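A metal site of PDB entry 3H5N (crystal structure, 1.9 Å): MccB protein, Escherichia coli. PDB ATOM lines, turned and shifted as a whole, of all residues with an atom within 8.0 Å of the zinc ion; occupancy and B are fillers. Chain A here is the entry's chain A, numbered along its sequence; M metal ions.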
ATOM      1  N   ASN A 227      27.601  31.132  32.082  1.00  0.00           N
ATOM      2  CA  ASN A 227      26.938  30.265  31.130  1.00  0.00           C
ATOM      3  C   ASN A 227      27.834  29.171  30.538  1.00  0.00           C
ATOM      4  O   ASN A 227      27.454  27.996  30.525  1.00  0.00           O
ATOM      5  CB  ASN A 227      26.338  31.093  29.997  1.00  0.00           C
ATOM      6  CG  ASN A 227      25.548  30.248  29.025  1.00  0.00           C
ATOM      7  OD1 ASN A 227      24.518  29.648  29.383  1.00  0.00           O
ATOM      8  ND2 ASN A 227      26.030  30.158  27.795  1.00  0.00           N
ATOM      9  N   VAL A 231      27.465  25.208  31.354  1.00  0.00           N
ATOM     10  CA  VAL A 231      27.222  24.270  30.250  1.00  0.00           C
ATOM     11  C   VAL A 231      28.253  23.142  30.282  1.00  0.00           C
ATOM     12  O   VAL A 231      27.909  21.965  30.191  1.00  0.00           O
ATOM     13  CB  VAL A 231      27.221  24.986  28.882  1.00  0.00           C
ATOM     14  CG1 VAL A 231      27.246  23.975  27.746  1.00  0.00           C
ATOM     15  CG2 VAL A 231      25.995  25.911  28.773  1.00  0.00           C
ATOM     16  N   TYR A 253      18.729  27.851  33.055  1.00  0.00           N
ATOM     17  CA  TYR A 253      19.438  26.866  32.255  1.00  0.00           C
ATOM     18  C   TYR A 253      19.397  25.517  32.954  1.00  0.00           C
ATOM     19  O   TYR A 253      19.749  25.410  34.125  1.00  0.00           O
ATOM     20  CB  TYR A 253      20.894  27.305  32.047  1.00  0.00           C
ATOM     21  CG  TYR A 253      21.721  26.207  31.394  1.00  0.00           C
ATOM     22  CD1 TYR A 253      21.490  25.841  30.062  1.00  0.00           C
ATOM     23  CD2 TYR A 253      22.690  25.532  32.119  1.00  0.00           C
ATOM     24  CE1 TYR A 253      22.225  24.832  29.472  1.00  0.00           C
ATOM     25  CE2 TYR A 253      23.428  24.513  31.529  1.00  0.00           C
ATOM     26  CZ  TYR A 253      23.183  24.174  30.209  1.00  0.00           C
ATOM     27  OH  TYR A 253      23.918  23.165  29.618  1.00  0.00           O
ATOM     28  N   THR A 258      17.038  22.888  28.140  1.00  0.00           N
ATOM     29  CA  THR A 258      16.746  24.271  27.773  1.00  0.00           C
ATOM     30  C   THR A 258      17.850  24.818  26.879  1.00  0.00           C
ATOM     31  O   THR A 258      18.934  24.227  26.782  1.00  0.00           O
ATOM     32  CB  THR A 258      16.658  25.214  29.031  1.00  0.00           C
ATOM     33  OG1 THR A 258      17.978  25.411  29.559  1.00  0.00           O
ATOM     34  CG2 THR A 258      15.735  24.671  30.116  1.00  0.00           C
ATOM     35  N   GLY A 259      17.599  25.949  26.236  1.00  0.00           N
ATOM     36  CA  GLY A 259      18.664  26.694  25.583  1.00  0.00           C
ATOM     37  C   GLY A 259      19.612  27.288  26.614  1.00  0.00           C
ATOM     38  O   GLY A 259      19.266  27.420  27.797  1.00  0.00           O
ATOM     39  N   CYS A 260      20.829  27.640  26.174  1.00  0.00           N
ATOM     40  CA  CYS A 260      21.742  28.364  27.056  1.00  0.00           C
ATOM     41  C   CYS A 260      21.686  29.844  26.705  1.00  0.00           C
ATOM     42  O   CYS A 260      20.946  30.248  25.790  1.00  0.00           O
ATOM     43  CB  CYS A 260      23.166  27.779  26.995  1.00  0.00           C
ATOM     44  SG  CYS A 260      24.252  28.353  25.672  1.00  0.00           S
ATOM     45  N   TYR A 261      22.446  30.648  27.437  1.00  0.00           N
ATOM     46  CA  TYR A 261      22.467  32.099  27.278  1.00  0.00           C
ATOM     47  C   TYR A 261      22.883  32.560  25.886  1.00  0.00           C
ATOM     48  O   TYR A 261      22.347  33.531  25.363  1.00  0.00           O
ATOM     49  CB  TYR A 261      23.391  32.718  28.325  1.00  0.00           C
ATOM     50  CG  TYR A 261      23.170  34.202  28.551  1.00  0.00           C
ATOM     51  CD1 TYR A 261      22.113  34.654  29.340  1.00  0.00           C
ATOM     52  CD2 TYR A 261      24.040  35.142  28.003  1.00  0.00           C
ATOM     53  CE1 TYR A 261      21.915  36.010  29.558  1.00  0.00           C
ATOM     54  CE2 TYR A 261      23.848  36.509  28.216  1.00  0.00           C
ATOM     55  CZ  TYR A 261      22.784  36.927  28.991  1.00  0.00           C
ATOM     56  OH  TYR A 261      22.573  38.268  29.216  1.00  0.00           O
ATOM     57  N   GLU A 262      23.844  31.855  25.303  1.00  0.00           N
ATOM     58  CA  GLU A 262      24.421  32.245  24.003  1.00  0.00           C
ATOM     59  C   GLU A 262      23.704  31.644  22.791  1.00  0.00           C
ATOM     60  O   GLU A 262      24.095  31.908  21.656  1.00  0.00           O
ATOM     61  CB  GLU A 262      25.930  31.942  23.973  1.00  0.00           C
ATOM     62  CG  GLU A 262      26.828  32.998  24.655  1.00  0.00           C
ATOM     63  CD  GLU A 262      27.104  32.734  26.149  1.00  0.00           C
ATOM     64  OE1 GLU A 262      27.689  31.676  26.485  1.00  0.00           O
ATOM     65  OE2 GLU A 262      26.771  33.600  26.981  1.00  0.00           O
ATOM     66  N   CYS A 263      22.649  30.851  23.029  1.00  0.00           N
ATOM     67  CA  CYS A 263      21.905  30.153  21.950  1.00  0.00           C
ATOM     68  C   CYS A 263      21.307  31.058  20.880  1.00  0.00           C
ATOM     69  O   CYS A 263      21.476  30.817  19.682  1.00  0.00           O
ATOM     70  CB  CYS A 263      20.809  29.247  22.523  1.00  0.00           C
ATOM     71  SG  CYS A 263      21.330  27.558  22.866  1.00  0.00           S
ATOM     72  N   GLN A 264      20.604  32.092  21.324  1.00  0.00           N
ATOM     73  CA  GLN A 264      19.872  32.995  20.443  1.00  0.00           C
ATOM     74  C   GLN A 264      20.571  34.360  20.308  1.00  0.00           C
ATOM     75  O   GLN A 264      19.926  35.357  19.972  1.00  0.00           O
ATOM     76  CB  GLN A 264      18.430  33.194  20.962  1.00  0.00           C
ATOM     77  CG  GLN A 264      17.619  31.911  21.158  1.00  0.00           C
ATOM     78  CD  GLN A 264      17.324  31.199  19.852  1.00  0.00           C
ATOM     79  OE1 GLN A 264      17.055  31.824  18.825  1.00  0.00           O
ATOM     80  NE2 GLN A 264      17.360  29.866  19.884  1.00  0.00           N
ATOM     81  N   LYS A 265      21.880  34.405  20.563  1.00  0.00           N
ATOM     82  CA  LYS A 265      22.620  35.666  20.613  1.00  0.00           C
ATOM     83  C   LYS A 265      22.609  36.433  19.284  1.00  0.00           C
ATOM     84  O   LYS A 265      22.846  35.863  18.223  1.00  0.00           O
ATOM     85  CB  LYS A 265      24.054  35.435  21.105  1.00  0.00           C
ATOM     86  N   MET A 340      14.907  32.039  24.516  1.00  0.00           N
ATOM     87  CA  MET A 340      16.255  31.558  24.724  1.00  0.00           C
ATOM     88  C   MET A 340      16.212  30.052  24.523  1.00  0.00           C
ATOM     89  O   MET A 340      16.823  29.294  25.274  1.00  0.00           O
ATOM     90  CB  MET A 340      16.755  31.867  26.150  1.00  0.00           C
ATOM     91  CG  MET A 340      16.471  33.261  26.673  1.00  0.00           C
ATOM     92  SD  MET A 340      17.849  34.417  26.581  1.00  0.00           S
ATOM     93  CE  MET A 340      19.173  33.500  27.333  1.00  0.00           C
ATOM     94  N   GLY A 341      15.463  29.628  23.499  1.00  0.00           N
ATOM     95  CA  GLY A 341      15.341  28.216  23.149  1.00  0.00           C
ATOM     96  C   GLY A 341      16.640  27.673  22.577  1.00  0.00           C
ATOM     97  O   GLY A 341      17.480  28.427  22.091  1.00  0.00           O
ATOM     98  N   ARG A 342      16.801  26.351  22.648  1.00  0.00           N
ATOM     99  CA  ARG A 342      18.023  25.685  22.233  1.00  0.00           C
ATOM    100  C   ARG A 342      18.251  25.807  20.738  1.00  0.00           C
ATOM    101  O   ARG A 342      17.310  25.678  19.952  1.00  0.00           O
ATOM    102  CB  ARG A 342      17.988  24.209  22.638  1.00  0.00           C
ATOM    103  CG  ARG A 342      19.342  23.524  22.716  1.00  0.00           C
ATOM    104  CD  ARG A 342      19.150  22.057  23.048  1.00  0.00           C
ATOM    105  NE  ARG A 342      20.400  21.370  23.358  1.00  0.00           N
ATOM    106  CZ  ARG A 342      20.469  20.120  23.828  1.00  0.00           C
ATOM    107  NH1 ARG A 342      19.355  19.423  24.050  1.00  0.00           N
ATOM    108  NH2 ARG A 342      21.647  19.576  24.099  1.00  0.00           N
ATOM    109  N   SER A 343      19.496  26.086  20.364  1.00  0.00           N
ATOM    110  CA  SER A 343      19.937  26.166  18.971  1.00  0.00           C
ATOM    111  C   SER A 343      20.997  25.089  18.758  1.00  0.00           C
ATOM    112  O   SER A 343      21.956  25.012  19.517  1.00  0.00           O
ATOM    113  CB  SER A 343      20.492  27.561  18.647  1.00  0.00           C
ATOM    114  OG  SER A 343      21.452  27.518  17.600  1.00  0.00           O
ATOM    115  N   PRO A 344      20.807  24.244  17.715  1.00  0.00           N
ATOM    116  CA  PRO A 344      21.768  23.165  17.453  1.00  0.00           C
ATOM    117  C   PRO A 344      23.104  23.767  17.046  1.00  0.00           C
ATOM    118  O   PRO A 344      24.166  23.184  17.280  1.00  0.00           O
ATOM    119  CB  PRO A 344      21.138  22.404  16.278  1.00  0.00           C
ATOM    120  CG  PRO A 344      19.739  22.924  16.136  1.00  0.00           C
ATOM    121  CD  PRO A 344      19.717  24.290  16.729  1.00  0.00           C
ATOM    122  N   VAL A 345      23.006  24.960  16.467  1.00  0.00           N
ATOM    123  CA  VAL A 345      24.119  25.738  15.952  1.00  0.00           C
ATOM    124  C   VAL A 345      25.018  26.299  17.060  1.00  0.00           C
ATOM    125  O   VAL A 345      26.222  26.457  16.851  1.00  0.00           O
ATOM    126  CB  VAL A 345      23.560  26.884  15.043  1.00  0.00           C
ATOM    127  CG1 VAL A 345      24.626  27.928  14.717  1.00  0.00           C
ATOM    128  CG2 VAL A 345      22.976  26.301  13.758  1.00  0.00           C
ATOM    129  N   CYS A 346      24.443  26.576  18.229  1.00  0.00           N
ATOM    130  CA  CYS A 346      25.137  27.249  19.330  1.00  0.00           C
ATOM    131  C   CYS A 346      26.586  26.832  19.533  1.00  0.00           C
ATOM    132  O   CYS A 346      26.901  25.643  19.612  1.00  0.00           O
ATOM    133  CB  CYS A 346      24.378  27.106  20.645  1.00  0.00           C
ATOM    134  SG  CYS A 346      25.220  27.944  22.031  1.00  0.00           S
ATOM    135  N   SER A 347      27.450  27.830  19.635  1.00  0.00           N
ATOM    136  CA  SER A 347      28.874  27.614  19.815  1.00  0.00           C
ATOM    137  C   SER A 347      29.238  27.121  21.217  1.00  0.00           C
ATOM    138  O   SER A 347      30.313  26.551  21.411  1.00  0.00           O
ATOM    139  CB  SER A 347      29.647  28.901  19.503  1.00  0.00           C
ATOM    140  OG  SER A 347      29.120  30.004  20.228  1.00  0.00           O
ATOM    141  N   VAL A 348      28.345  27.339  22.178  1.00  0.00           N
ATOM    142  CA  VAL A 348      28.635  26.959  23.567  1.00  0.00           C
ATOM    143  C   VAL A 348      28.097  25.572  23.938  1.00  0.00           C
ATOM    144  O   VAL A 348      28.839  24.729  24.428  1.00  0.00           O
ATOM    145  CB  VAL A 348      28.150  28.026  24.584  1.00  0.00           C
ATOM    146  CG1 VAL A 348      28.481  27.598  26.009  1.00  0.00           C
ATOM    147  CG2 VAL A 348      28.773  29.370  24.275  1.00  0.00           C
ATOM    148  N   CYS A 349      26.800  25.354  23.717  1.00  0.00           N
ATOM    149  CA  CYS A 349      26.160  24.103  24.103  1.00  0.00           C
ATOM    150  C   CYS A 349      25.794  23.236  22.892  1.00  0.00           C
ATOM    151  O   CYS A 349      25.273  22.128  23.049  1.00  0.00           O
ATOM    152  CB  CYS A 349      24.918  24.382  24.945  1.00  0.00           C
ATOM    153  SG  CYS A 349      23.546  25.075  24.021  1.00  0.00           S
ATOM    154  N   GLY A 350      26.061  23.752  21.696  1.00  0.00           N
ATOM    155  CA  GLY A 350      25.805  23.015  20.466  1.00  0.00           C
ATOM    156  C   GLY A 350      27.065  22.377  19.946  1.00  0.00           C
ATOM    157  O   GLY A 350      27.473  21.298  20.382  1.00  0.00           O
HETATM  158 ZN    ZN M   1      23.567  27.364  23.553  1.00  0.00          ZN
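The backbone NH of Val 348 lies close to the side-chain sulfur of Cys 346 (3.2 Å).
N of Cys 346 is in hydrogen-bond range of OG of Ser 343 (3.2 Å).
N of Ser 343 lies close to SG of Cys 263, at 3.4 Å.
SG of Cys 260 lies close to N of Glu 262 (3.5 Å).
The side-chain amide nitrogen of Asn 227 lies close to the side-chain sulfur of Cys 260 (3.3 Å).
The zinc ion is bound by the side-chain sulfur of Cys 346 (2.3 Å), the side-chain sulfur of Cys 349 (2.3 Å), the side-chain sulfur of Cys 263 (2.3 Å) and the side-chain sulfur of Cys 260 (2.4 Å).
The zinc ion has four donor atoms within binding distance.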
